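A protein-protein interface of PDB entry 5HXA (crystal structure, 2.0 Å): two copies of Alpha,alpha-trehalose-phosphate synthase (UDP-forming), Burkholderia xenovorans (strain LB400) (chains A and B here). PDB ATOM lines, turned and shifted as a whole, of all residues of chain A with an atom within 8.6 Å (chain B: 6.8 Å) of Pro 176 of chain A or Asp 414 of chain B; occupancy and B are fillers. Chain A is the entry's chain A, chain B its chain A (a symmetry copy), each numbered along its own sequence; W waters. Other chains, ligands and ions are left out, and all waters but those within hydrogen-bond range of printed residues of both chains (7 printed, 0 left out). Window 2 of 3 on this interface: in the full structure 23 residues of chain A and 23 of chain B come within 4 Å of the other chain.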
ATOM      1  N   PHE A  88     -29.311  27.322 -12.772  1.00  0.00           N
ATOM      2  CA  PHE A  88     -28.718  26.123 -13.357  1.00  0.00           C
ATOM      3  C   PHE A  88     -27.308  26.385 -13.875  1.00  0.00           C
ATOM      4  O   PHE A  88     -26.407  25.575 -13.645  1.00  0.00           O
ATOM      5  CB  PHE A  88     -29.599  25.546 -14.464  1.00  0.00           C
ATOM      6  CG  PHE A  88     -29.157  24.174 -14.900  1.00  0.00           C
ATOM      7  CD1 PHE A  88     -29.363  23.069 -14.068  1.00  0.00           C
ATOM      8  CD2 PHE A  88     -28.490  23.994 -16.104  1.00  0.00           C
ATOM      9  CE1 PHE A  88     -28.934  21.804 -14.447  1.00  0.00           C
ATOM     10  CE2 PHE A  88     -28.061  22.729 -16.491  1.00  0.00           C
ATOM     11  CZ  PHE A  88     -28.278  21.636 -15.663  1.00  0.00           C
ATOM     12  N   THR A  92     -25.287  25.075 -10.634  1.00  0.00           N
ATOM     13  CA  THR A  92     -25.174  23.650 -10.945  1.00  0.00           C
ATOM     14  C   THR A  92     -23.998  23.375 -11.869  1.00  0.00           C
ATOM     15  O   THR A  92     -23.077  22.652 -11.479  1.00  0.00           O
ATOM     16  CB  THR A  92     -26.469  23.113 -11.567  1.00  0.00           C
ATOM     17  OG1 THR A  92     -27.576  23.416 -10.709  1.00  0.00           O
ATOM     18  CG2 THR A  92     -26.384  21.583 -11.766  1.00  0.00           C
ATOM     19  N   LEU A  93     -23.990  23.946 -13.076  1.00  0.00           N
ATOM     20  CA  LEU A  93     -22.953  23.602 -14.045  1.00  0.00           C
ATOM     21  C   LEU A  93     -21.583  24.108 -13.605  1.00  0.00           C
ATOM     22  O   LEU A  93     -20.601  23.353 -13.619  1.00  0.00           O
ATOM     23  CB  LEU A  93     -23.310  24.159 -15.431  1.00  0.00           C
ATOM     24  CG  LEU A  93     -24.562  23.584 -16.106  1.00  0.00           C
ATOM     25  CD1 LEU A  93     -24.796  24.229 -17.479  1.00  0.00           C
ATOM     26  CD2 LEU A  93     -24.481  22.063 -16.224  1.00  0.00           C
ATOM     27  N   THR A  96     -19.876  22.033 -10.664  1.00  0.00           N
ATOM     28  CA  THR A  96     -19.588  20.660 -11.084  1.00  0.00           C
ATOM     29  C   THR A  96     -18.508  20.602 -12.164  1.00  0.00           C
ATOM     30  O   THR A  96     -17.609  19.749 -12.110  1.00  0.00           O
ATOM     31  CB  THR A  96     -20.870  19.986 -11.580  1.00  0.00           C
ATOM     32  OG1 THR A  96     -21.839  20.005 -10.532  1.00  0.00           O
ATOM     33  CG2 THR A  96     -20.596  18.525 -11.953  1.00  0.00           C
ATOM     34  N   SER A 104     -22.442  22.029  -5.709  1.00  0.00           N
ATOM     35  CA  SER A 104     -23.522  22.112  -6.679  1.00  0.00           C
ATOM     36  C   SER A 104     -24.867  21.858  -6.008  1.00  0.00           C
ATOM     37  O   SER A 104     -24.969  21.121  -5.027  1.00  0.00           O
ATOM     38  CB  SER A 104     -23.296  21.095  -7.800  1.00  0.00           C
ATOM     39  OG  SER A 104     -24.259  21.204  -8.841  1.00  0.00           O
ATOM     40  N   ARG A 105     -25.904  22.486  -6.543  1.00  0.00           N
ATOM     41  CA  ARG A 105     -27.269  22.220  -6.118  1.00  0.00           C
ATOM     42  C   ARG A 105     -28.120  22.101  -7.368  1.00  0.00           C
ATOM     43  O   ARG A 105     -27.968  22.895  -8.299  1.00  0.00           O
ATOM     44  CB  ARG A 105     -27.805  23.336  -5.205  1.00  0.00           C
ATOM     45  CG  ARG A 105     -27.037  23.495  -3.892  1.00  0.00           C
ATOM     46  CD  ARG A 105     -27.162  22.273  -2.978  1.00  0.00           C
ATOM     47  NE  ARG A 105     -26.488  22.476  -1.692  1.00  0.00           N
ATOM     48  CZ  ARG A 105     -25.196  22.237  -1.473  1.00  0.00           C
ATOM     49  NH1 ARG A 105     -24.424  21.778  -2.452  1.00  0.00           N
ATOM     50  NH2 ARG A 105     -24.673  22.453  -0.274  1.00  0.00           N
ATOM     51  N   TYR A 106     -29.001  21.113  -7.402  1.00  0.00           N
ATOM     52  CA  TYR A 106     -29.845  20.893  -8.566  1.00  0.00           C
ATOM     53  C   TYR A 106     -31.293  21.174  -8.205  1.00  0.00           C
ATOM     54  O   TYR A 106     -31.777  20.745  -7.153  1.00  0.00           O
ATOM     55  CB  TYR A 106     -29.713  19.465  -9.109  1.00  0.00           C
ATOM     56  CG  TYR A 106     -30.667  19.221 -10.257  1.00  0.00           C
ATOM     57  CD1 TYR A 106     -30.478  19.861 -11.484  1.00  0.00           C
ATOM     58  CD2 TYR A 106     -31.776  18.398 -10.105  1.00  0.00           C
ATOM     59  CE1 TYR A 106     -31.357  19.667 -12.536  1.00  0.00           C
ATOM     60  CE2 TYR A 106     -32.659  18.193 -11.152  1.00  0.00           C
ATOM     61  CZ  TYR A 106     -32.443  18.833 -12.365  1.00  0.00           C
ATOM     62  OH  TYR A 106     -33.318  18.645 -13.406  1.00  0.00           O
ATOM     63  N   ASP A 107     -31.980  21.894  -9.083  1.00  0.00           N
ATOM     64  CA  ASP A 107     -33.391  22.181  -8.896  1.00  0.00           C
ATOM     65  C   ASP A 107     -34.100  22.057 -10.237  1.00  0.00           C
ATOM     66  O   ASP A 107     -33.688  22.676 -11.225  1.00  0.00           O
ATOM     67  CB  ASP A 107     -33.597  23.576  -8.301  1.00  0.00           C
ATOM     68  CG  ASP A 107     -35.060  23.878  -8.033  1.00  0.00           C
ATOM     69  OD1 ASP A 107     -35.575  23.447  -6.980  1.00  0.00           O
ATOM     70  OD2 ASP A 107     -35.693  24.529  -8.882  1.00  0.00           O
ATOM     71  N   ARG A 108     -35.153  21.241 -10.268  1.00  0.00           N
ATOM     72  CA  ARG A 108     -35.855  20.981 -11.522  1.00  0.00           C
ATOM     73  C   ARG A 108     -36.401  22.256 -12.145  1.00  0.00           C
ATOM     74  O   ARG A 108     -36.409  22.394 -13.371  1.00  0.00           O
ATOM     75  CB  ARG A 108     -37.006  20.017 -11.291  1.00  0.00           C
ATOM     76  CG  ARG A 108     -36.609  18.601 -11.163  1.00  0.00           C
ATOM     77  CD  ARG A 108     -37.858  17.801 -10.874  1.00  0.00           C
ATOM     78  NE  ARG A 108     -37.552  16.384 -10.771  1.00  0.00           N
ATOM     79  CZ  ARG A 108     -38.435  15.468 -10.399  1.00  0.00           C
ATOM     80  NH1 ARG A 108     -39.682  15.827 -10.082  1.00  0.00           N
ATOM     81  NH2 ARG A 108     -38.062  14.203 -10.326  1.00  0.00           N
ATOM     82  N   TYR A 111     -33.618  24.155 -13.828  1.00  0.00           N
ATOM     83  CA  TYR A 111     -33.253  23.514 -15.090  1.00  0.00           C
ATOM     84  C   TYR A 111     -34.319  23.749 -16.157  1.00  0.00           C
ATOM     85  O   TYR A 111     -33.991  23.939 -17.335  1.00  0.00           O
ATOM     86  CB  TYR A 111     -33.003  22.009 -14.879  1.00  0.00           C
ATOM     87  CG  TYR A 111     -32.652  21.275 -16.167  1.00  0.00           C
ATOM     88  CD1 TYR A 111     -31.561  21.674 -16.944  1.00  0.00           C
ATOM     89  CD2 TYR A 111     -33.412  20.196 -16.614  1.00  0.00           C
ATOM     90  CE1 TYR A 111     -31.243  21.019 -18.127  1.00  0.00           C
ATOM     91  CE2 TYR A 111     -33.099  19.534 -17.804  1.00  0.00           C
ATOM     92  CZ  TYR A 111     -32.014  19.954 -18.556  1.00  0.00           C
ATOM     93  OH  TYR A 111     -31.694  19.304 -19.736  1.00  0.00           O
ATOM     94  N   VAL A 171     -17.825  12.457 -12.826  1.00  0.00           N
ATOM     95  CA  VAL A 171     -18.213  13.729 -12.223  1.00  0.00           C
ATOM     96  C   VAL A 171     -19.406  14.334 -12.943  1.00  0.00           C
ATOM     97  O   VAL A 171     -20.342  14.810 -12.296  1.00  0.00           O
ATOM     98  CB  VAL A 171     -17.008  14.695 -12.208  1.00  0.00           C
ATOM     99  CG1 VAL A 171     -17.430  16.120 -11.786  1.00  0.00           C
ATOM    100  CG2 VAL A 171     -15.914  14.157 -11.286  1.00  0.00           C
ATOM    101  N   LEU A 172     -19.377  14.315 -14.281  1.00  0.00           N
ATOM    102  CA  LEU A 172     -20.502  14.806 -15.075  1.00  0.00           C
ATOM    103  C   LEU A 172     -21.816  14.136 -14.687  1.00  0.00           C
ATOM    104  O   LEU A 172     -22.866  14.791 -14.650  1.00  0.00           O
ATOM    105  CB  LEU A 172     -20.234  14.569 -16.569  1.00  0.00           C
ATOM    106  CG  LEU A 172     -21.336  15.060 -17.516  1.00  0.00           C
ATOM    107  CD1 LEU A 172     -21.280  16.570 -17.597  1.00  0.00           C
ATOM    108  CD2 LEU A 172     -21.186  14.439 -18.896  1.00  0.00           C
ATOM    109  N   ARG A 173     -21.786  12.826 -14.416  1.00  0.00           N
ATOM    110  CA  ARG A 173     -23.038  12.115 -14.183  1.00  0.00           C
ATOM    111  C   ARG A 173     -23.696  12.491 -12.861  1.00  0.00           C
ATOM    112  O   ARG A 173     -24.843  12.087 -12.629  1.00  0.00           O
ATOM    113  CB  ARG A 173     -22.819  10.596 -14.261  1.00  0.00           C
ATOM    114  CG  ARG A 173     -21.965   9.963 -13.152  1.00  0.00           C
ATOM    115  CD  ARG A 173     -21.573   8.518 -13.548  1.00  0.00           C
ATOM    116  NE  ARG A 173     -20.966   7.755 -12.457  1.00  0.00           N
ATOM    117  CZ  ARG A 173     -21.623   6.879 -11.700  1.00  0.00           C
ATOM    118  NH1 ARG A 173     -22.914   6.649 -11.914  1.00  0.00           N
ATOM    119  NH2 ARG A 173     -20.996   6.236 -10.725  1.00  0.00           N
ATOM    120  N   THR A 174     -23.026  13.272 -12.008  1.00  0.00           N
ATOM    121  CA  THR A 174     -23.693  13.768 -10.807  1.00  0.00           C
ATOM    122  C   THR A 174     -24.714  14.857 -11.134  1.00  0.00           C
ATOM    123  O   THR A 174     -25.611  15.111 -10.323  1.00  0.00           O
ATOM    124  CB  THR A 174     -22.677  14.286  -9.772  1.00  0.00           C
ATOM    125  OG1 THR A 174     -21.980  15.433 -10.280  1.00  0.00           O
ATOM    126  CG2 THR A 174     -21.667  13.187  -9.404  1.00  0.00           C
ATOM    127  N   ILE A 175     -24.611  15.494 -12.298  1.00  0.00           N
ATOM    128  CA  ILE A 175     -25.628  16.451 -12.753  1.00  0.00           C
ATOM    129  C   ILE A 175     -26.838  15.656 -13.242  1.00  0.00           C
ATOM    130  O   ILE A 175     -26.715  14.895 -14.212  1.00  0.00           O
ATOM    131  CB  ILE A 175     -25.084  17.354 -13.870  1.00  0.00           C
ATOM    132  CG1 ILE A 175     -23.907  18.200 -13.371  1.00  0.00           C
ATOM    133  CG2 ILE A 175     -26.199  18.227 -14.460  1.00  0.00           C
ATOM    134  CD1 ILE A 175     -23.064  18.761 -14.529  1.00  0.00           C
ATOM    135  N   PRO A 176     -28.010  15.780 -12.627  1.00  0.00           N
ATOM    136  CA  PRO A 176     -29.090  14.814 -12.895  1.00  0.00           C
ATOM    137  C   PRO A 176     -29.493  14.762 -14.365  1.00  0.00           C
ATOM    138  O   PRO A 176     -29.608  13.660 -14.915  1.00  0.00           O
ATOM    139  CB  PRO A 176     -30.229  15.292 -11.977  1.00  0.00           C
ATOM    140  CG  PRO A 176     -29.477  15.857 -10.793  1.00  0.00           C
ATOM    141  CD  PRO A 176     -28.307  16.602 -11.436  1.00  0.00           C
ATOM    142  N   PRO A 177     -29.690  15.906 -15.072  1.00  0.00           N
ATOM    143  CA  PRO A 177     -30.022  15.792 -16.509  1.00  0.00           C
ATOM    144  C   PRO A 177     -28.825  15.707 -17.457  1.00  0.00           C
ATOM    145  O   PRO A 177     -28.944  16.108 -18.622  1.00  0.00           O
ATOM    146  CB  PRO A 177     -30.825  17.070 -16.779  1.00  0.00           C
ATOM    147  CG  PRO A 177     -30.186  18.076 -15.853  1.00  0.00           C
ATOM    148  CD  PRO A 177     -29.862  17.295 -14.592  1.00  0.00           C
ATOM    149  N   HIS A 178     -27.687  15.171 -17.000  1.00  0.00           N
ATOM    150  CA  HIS A 178     -26.480  15.194 -17.828  1.00  0.00           C
ATOM    151  C   HIS A 178     -26.682  14.488 -19.165  1.00  0.00           C
ATOM    152  O   HIS A 178     -26.120  14.913 -20.180  1.00  0.00           O
ATOM    153  CB  HIS A 178     -25.300  14.568 -17.078  1.00  0.00           C
ATOM    154  CG  HIS A 178     -25.472  13.111 -16.788  1.00  0.00           C
ATOM    155  ND1 HIS A 178     -26.168  12.648 -15.691  1.00  0.00           N
ATOM    156  CD2 HIS A 178     -25.034  12.012 -17.448  1.00  0.00           C
ATOM    157  CE1 HIS A 178     -26.161  11.325 -15.695  1.00  0.00           C
ATOM    158  NE2 HIS A 178     -25.481  10.916 -16.752  1.00  0.00           N
ATOM    159  N   GLU A 179     -27.472  13.408 -19.201  1.00  0.00           N
ATOM    160  CA  GLU A 179     -27.630  12.695 -20.473  1.00  0.00           C
ATOM    161  C   GLU A 179     -28.336  13.553 -21.519  1.00  0.00           C
ATOM    162  O   GLU A 179     -27.948  13.561 -22.697  1.00  0.00           O
ATOM    163  CB  GLU A 179     -28.376  11.381 -20.252  1.00  0.00           C
ATOM    164  CG  GLU A 179     -27.674  10.495 -19.259  1.00  0.00           C
ATOM    165  CD  GLU A 179     -27.933   9.030 -19.498  1.00  0.00           C
ATOM    166  OE1 GLU A 179     -26.952   8.252 -19.530  1.00  0.00           O
ATOM    167  OE2 GLU A 179     -29.115   8.663 -19.666  1.00  0.00           O
ATOM    168  N   GLU A 180     -29.372  14.285 -21.110  1.00  0.00           N
ATOM    169  CA  GLU A 180     -30.079  15.157 -22.042  1.00  0.00           C
ATOM    170  C   GLU A 180     -29.171  16.278 -22.543  1.00  0.00           C
ATOM    171  O   GLU A 180     -29.253  16.689 -23.712  1.00  0.00           O
ATOM    172  CB  GLU A 180     -31.324  15.720 -21.341  1.00  0.00           C
ATOM    173  CG  GLU A 180     -32.149  16.680 -22.157  1.00  0.00           C
ATOM    174  CD  GLU A 180     -33.480  17.003 -21.492  1.00  0.00           C
ATOM    175  OE1 GLU A 180     -33.486  17.359 -20.288  1.00  0.00           O
ATOM    176  OE2 GLU A 180     -34.519  16.882 -22.176  1.00  0.00           O
ATOM    177  N   LEU A 181     -28.281  16.766 -21.678  1.00  0.00           N
ATOM    178  CA  LEU A 181     -27.375  17.847 -22.054  1.00  0.00           C
ATOM    179  C   LEU A 181     -26.360  17.390 -23.094  1.00  0.00           C
ATOM    180  O   LEU A 181     -26.102  18.101 -24.067  1.00  0.00           O
ATOM    181  CB  LEU A 181     -26.665  18.381 -20.810  1.00  0.00           C
ATOM    182  CG  LEU A 181     -27.541  19.200 -19.840  1.00  0.00           C
ATOM    183  CD1 LEU A 181     -26.799  19.462 -18.526  1.00  0.00           C
ATOM    184  CD2 LEU A 181     -28.022  20.513 -20.473  1.00  0.00           C
ATOM    185  N   ALA B 285     -34.384  14.684   1.249  1.00  0.00           N
ATOM    186  CA  ALA B 285     -35.339  14.064   0.328  1.00  0.00           C
ATOM    187  C   ALA B 285     -36.529  13.480   1.083  1.00  0.00           C
ATOM    188  O   ALA B 285     -37.646  13.449   0.552  1.00  0.00           O
ATOM    189  CB  ALA B 285     -34.657  12.982  -0.517  1.00  0.00           C
ATOM    190  N   ARG B 288     -38.635  16.361   1.498  1.00  0.00           N
ATOM    191  CA  ARG B 288     -39.339  16.645   0.251  1.00  0.00           C
ATOM    192  C   ARG B 288     -40.516  15.690   0.056  1.00  0.00           C
ATOM    193  O   ARG B 288     -41.571  16.087  -0.457  1.00  0.00           O
ATOM    194  CB  ARG B 288     -38.371  16.568  -0.940  1.00  0.00           C
ATOM    195  CG  ARG B 288     -38.984  17.067  -2.257  1.00  0.00           C
ATOM    196  CD  ARG B 288     -37.912  17.533  -3.256  1.00  0.00           C
ATOM    197  NE  ARG B 288     -37.137  18.668  -2.743  1.00  0.00           N
ATOM    198  CZ  ARG B 288     -36.232  19.341  -3.447  1.00  0.00           C
ATOM    199  NH1 ARG B 288     -35.992  19.019  -4.710  1.00  0.00           N
ATOM    200  NH2 ARG B 288     -35.583  20.359  -2.897  1.00  0.00           N
ATOM    201  N   GLN B 396     -27.062   5.397  -7.405  1.00  0.00           N
ATOM    202  CA  GLN B 396     -26.281   4.875  -8.520  1.00  0.00           C
ATOM    203  C   GLN B 396     -24.778   4.969  -8.276  1.00  0.00           C
ATOM    204  O   GLN B 396     -24.005   4.483  -9.105  1.00  0.00           O
ATOM    205  CB  GLN B 396     -26.658   5.603  -9.820  1.00  0.00           C
ATOM    206  CG  GLN B 396     -26.609   7.099  -9.785  1.00  0.00           C
ATOM    207  CD  GLN B 396     -27.411   7.730 -10.931  1.00  0.00           C
ATOM    208  OE1 GLN B 396     -28.337   7.126 -11.470  1.00  0.00           O
ATOM    209  NE2 GLN B 396     -27.043   8.934 -11.305  1.00  0.00           N
ATOM    210  N   VAL B 410     -31.449   5.585  -7.899  1.00  0.00           N
ATOM    211  CA  VAL B 410     -31.617   7.032  -7.944  1.00  0.00           C
ATOM    212  C   VAL B 410     -30.264   7.736  -7.946  1.00  0.00           C
ATOM    213  O   VAL B 410     -29.241   7.198  -7.512  1.00  0.00           O
ATOM    214  CB  VAL B 410     -32.475   7.559  -6.763  1.00  0.00           C
ATOM    215  CG1 VAL B 410     -33.901   6.984  -6.829  1.00  0.00           C
ATOM    216  CG2 VAL B 410     -31.808   7.242  -5.408  1.00  0.00           C
ATOM    217  N   ASN B 411     -30.284   8.964  -8.460  1.00  0.00           N
ATOM    218  CA  ASN B 411     -29.150   9.871  -8.370  1.00  0.00           C
ATOM    219  C   ASN B 411     -29.311  10.665  -7.078  1.00  0.00           C
ATOM    220  O   ASN B 411     -30.257  11.460  -6.969  1.00  0.00           O
ATOM    221  CB  ASN B 411     -29.129  10.800  -9.573  1.00  0.00           C
ATOM    222  CG  ASN B 411     -27.900  11.693  -9.607  1.00  0.00           C
ATOM    223  OD1 ASN B 411     -27.285  11.982  -8.570  1.00  0.00           O
ATOM    224  ND2 ASN B 411     -27.548  12.145 -10.793  1.00  0.00           N
ATOM    225  N   PRO B 412     -28.449  10.479  -6.071  1.00  0.00           N
ATOM    226  CA  PRO B 412     -28.673  11.169  -4.789  1.00  0.00           C
ATOM    227  C   PRO B 412     -28.499  12.675  -4.887  1.00  0.00           C
ATOM    228  O   PRO B 412     -28.899  13.387  -3.953  1.00  0.00           O
ATOM    229  CB  PRO B 412     -27.629  10.531  -3.854  1.00  0.00           C
ATOM    230  CG  PRO B 412     -26.500  10.164  -4.787  1.00  0.00           C
ATOM    231  CD  PRO B 412     -27.203   9.694  -6.071  1.00  0.00           C
ATOM    232  N   PHE B 413     -27.927  13.189  -5.978  1.00  0.00           N
ATOM    233  CA  PHE B 413     -27.872  14.634  -6.180  1.00  0.00           C
ATOM    234  C   PHE B 413     -29.199  15.208  -6.670  1.00  0.00           C
ATOM    235  O   PHE B 413     -29.276  16.412  -6.923  1.00  0.00           O
ATOM    236  CB  PHE B 413     -26.755  14.988  -7.173  1.00  0.00           C
ATOM    237  CG  PHE B 413     -25.380  14.657  -6.666  1.00  0.00           C
ATOM    238  CD1 PHE B 413     -24.860  13.377  -6.811  1.00  0.00           C
ATOM    239  CD2 PHE B 413     -24.616  15.614  -6.016  1.00  0.00           C
ATOM    240  CE1 PHE B 413     -23.593  13.063  -6.321  1.00  0.00           C
ATOM    241  CE2 PHE B 413     -23.351  15.307  -5.531  1.00  0.00           C
ATOM    242  CZ  PHE B 413     -22.843  14.026  -5.682  1.00  0.00           C
ATOM    243  N   ASP B 414     -30.224  14.372  -6.833  1.00  0.00           N
ATOM    244  CA  ASP B 414     -31.547  14.765  -7.312  1.00  0.00           C
ATOM    245  C   ASP B 414     -32.521  14.512  -6.160  1.00  0.00           C
ATOM    246  O   ASP B 414     -33.069  13.415  -6.028  1.00  0.00           O
ATOM    247  CB  ASP B 414     -31.927  13.967  -8.592  1.00  0.00           C
ATOM    248  CG  ASP B 414     -33.178  14.497  -9.270  1.00  0.00           C
ATOM    249  OD1 ASP B 414     -33.955  15.226  -8.626  1.00  0.00           O
ATOM    250  OD2 ASP B 414     -33.383  14.179 -10.457  1.00  0.00           O
ATOM    251  N   LEU B 415     -32.726  15.526  -5.311  1.00  0.00           N
ATOM    252  CA  LEU B 415     -33.594  15.334  -4.149  1.00  0.00           C
ATOM    253  C   LEU B 415     -35.011  14.952  -4.566  1.00  0.00           C
ATOM    254  O   LEU B 415     -35.663  14.129  -3.904  1.00  0.00           O
ATOM    255  CB  LEU B 415     -33.609  16.599  -3.286  1.00  0.00           C
ATOM    256  CG  LEU B 415     -32.272  16.966  -2.636  1.00  0.00           C
ATOM    257  CD1 LEU B 415     -32.423  18.231  -1.796  1.00  0.00           C
ATOM    258  CD2 LEU B 415     -31.728  15.808  -1.780  1.00  0.00           C
ATOM    259  N   SER B 416     -35.512  15.536  -5.658  1.00  0.00           N
ATOM    260  CA  SER B 416     -36.870  15.232  -6.095  1.00  0.00           C
ATOM    261  C   SER B 416     -36.995  13.784  -6.561  1.00  0.00           C
ATOM    262  O   SER B 416     -37.990  13.115  -6.257  1.00  0.00           O
ATOM    263  CB  SER B 416     -37.303  16.184  -7.213  1.00  0.00           C
ATOM    264  OG  SER B 416     -37.501  17.492  -6.710  1.00  0.00           O
ATOM    265  N   GLN B 417     -36.012  13.289  -7.320  1.00  0.00           N
ATOM    266  CA  GLN B 417     -36.052  11.885  -7.720  1.00  0.00           C
ATOM    267  C   GLN B 417     -36.026  10.957  -6.505  1.00  0.00           C
ATOM    268  O   GLN B 417     -36.763   9.966  -6.459  1.00  0.00           O
ATOM    269  CB  GLN B 417     -34.888  11.555  -8.655  1.00  0.00           C
ATOM    270  CG  GLN B 417     -34.894  10.082  -9.088  1.00  0.00           C
ATOM    271  CD  GLN B 417     -33.672   9.690  -9.900  1.00  0.00           C
ATOM    272  OE1 GLN B 417     -32.575  10.181  -9.666  1.00  0.00           O
ATOM    273  NE2 GLN B 417     -33.863   8.797 -10.852  1.00  0.00           N
ATOM    274  N   MET B 418     -35.181  11.257  -5.512  1.00  0.00           N
ATOM    275  CA  MET B 418     -35.136  10.422  -4.311  1.00  0.00           C
ATOM    276  C   MET B 418     -36.465  10.455  -3.563  1.00  0.00           C
ATOM    277  O   MET B 418     -36.944   9.416  -3.099  1.00  0.00           O
ATOM    278  CB  MET B 418     -33.996  10.867  -3.385  1.00  0.00           C
ATOM    279  CG  MET B 418     -32.608  10.569  -3.952  1.00  0.00           C
ATOM    280  SD  MET B 418     -31.434   9.960  -2.715  1.00  0.00           S
ATOM    281  CE  MET B 418     -31.203  11.441  -1.707  1.00  0.00           C
ATOM    282  N   ALA B 419     -37.063  11.646  -3.411  1.00  0.00           N
ATOM    283  CA  ALA B 419     -38.357  11.738  -2.743  1.00  0.00           C
ATOM    284  C   ALA B 419     -39.405  10.916  -3.474  1.00  0.00           C
ATOM    285  O   ALA B 419     -40.253  10.269  -2.850  1.00  0.00           O
ATOM    286  CB  ALA B 419     -38.805  13.198  -2.658  1.00  0.00           C
HETATM  287  O   HOH W   1     -31.562  17.980  -6.098  1.00  0.00           O
HETATM  288  O   HOH W   2     -29.294  11.599 -13.089  1.00  0.00           O
HETATM  289  O   HOH W   3     -27.291  18.512  -6.694  1.00  0.00           O
HETATM  290  O   HOH W   4     -35.451  14.724 -11.685  1.00  0.00           O
HETATM  291  O   HOH W   5     -33.959  21.150  -5.301  1.00  0.00           O
HETATM  292  O   HOH W   6     -35.693  19.817  -7.882  1.00  0.00           O
HETATM  293  O   HOH W   7     -22.098   3.709 -10.788  1.00  0.00           O
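No position is printed for both chains.
The side-chain amide nitrogen (ND2) of Asn 411 of chain B sits at hydrogen-bond distance from the backbone carbonyl oxygen (O) of Arg 173 of chain A, 3.3 Å away.
Phe 413 of chain B touches Tyr 106 of chain A.
Ser 416 of chain B touches Arg 108 of chain A (CB to CZ, 3.5 Å).
Arg 108 of chain A touches Gln 417 of chain B (NH2 to N, 3.8 Å).
Arg 173 of chain A touches Gln 396 of chain B.
Thr 174 of chain A touches Asn 411 of chain B (O to ND2, 3.6 Å).
O of Thr 174 of chain A touches CB of Phe 413 of chain B, 3.4 Å away.
Asn 411 of chain B touches Pro 176 of chain A (ND2 to CA, 3.7 Å).
Pro 176 of chain A touches Phe 413 of chain B.
Pro 176 of chain A touches Asp 414 of chain B.
Hydrophobic or aromatic side chains of chain A within 4 Å of the printed part of chain B: Tyr 106 and Pro 176.
Among the printed residues, 10 pairs touch across the chains.
Among the printed residues, no Asp or Glu carboxylate lies within 4 Å of a Lys or Arg side-chain nitrogen of the other chain.
Of the printed residues of chain B, Pro 176 of chain A touches Asn 411, Phe 413 and Asp 414.
Of the printed residues of chain A, Asp 414 of chain B touches Pro 176 (3.7 Å).
Of the printed residues of chain A, Asn 411 of chain B touches Arg 173, Thr 174 and Pro 176.
Of the printed residues of chain B, Arg 173 of chain A touches Gln 396 (3.7 Å) and Asn 411 (3.3 Å).
Of the printed residues of chain B, Arg 108 of chain A touches Ser 416 and Gln 417.
Of the printed residues of chain A, Gln 417 of chain B touches Arg 108.
The nearest residue of chain A that does not touch Asp 414 of chain B is Tyr 106 of chain A (4.1 Å).
The nearest printed residue of chain B that does not touch Arg 108 of chain A is Asp 414 of chain B (4.3 Å).
OD1 of Asp 414 of chain B is in hydrogen-bond range of N of Gln 417 of chain B (3.1 Å).
The backbone NH (N) of Ser 416 of chain B lies close to the side-chain carboxylate (OD1) of Asp 414 of chain B (3.4 Å).
The backbone carbonyl oxygen (O) of Val 171 of chain A lies within hydrogen-bond range of the side-chain hydroxyl (OG1) of Thr 174 of chain A, at 2.7 Å.
OE1 of Gln 417 of chain B is in hydrogen-bond range of N of Asn 411 of chain B.
A ring nitrogen (ND1) of His 178 of chain A is in hydrogen-bond range of the backbone carbonyl oxygen (O) of Arg 173 of chain A (3.4 Å).
N of Phe 413 of chain B is in hydrogen-bond range of OD1 of Asn 411 of chain B (2.9 Å).
Water W4 bridges OD2 of Asp 414 of chain B (2.5 Å) and NE of Arg 108 of chain A (2.8 Å).
Water W7 bridges the backbone carbonyl oxygen of Gln 396 of chain B and the guanidinium group of Arg 173 of chain A.
Water W2 lies within hydrogen-bond range of the backbone carbonyl oxygen (O) of Pro 176 of chain A and the side-chain amide nitrogen (ND2) of Asn 411 of chain B.
Water W1 lies within hydrogen-bond range of N of Leu 415 of chain B, O of Phe 413 of chain B and O of Tyr 106 of chain A.
Water W6 lies within hydrogen-bond range of the backbone NH of Arg 108 of chain A (2.8 Å), the side-chain hydroxyl of Ser 416 of chain B (3.2 Å) and the guanidinium group of Arg 288 of chain B (3.3 Å).
Water W3 lies within hydrogen-bond range of the backbone carbonyl oxygen (O) of Phe 413 of chain B (2.9 Å) and the backbone NH (N) of Tyr 106 of chain A (3.2 Å).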
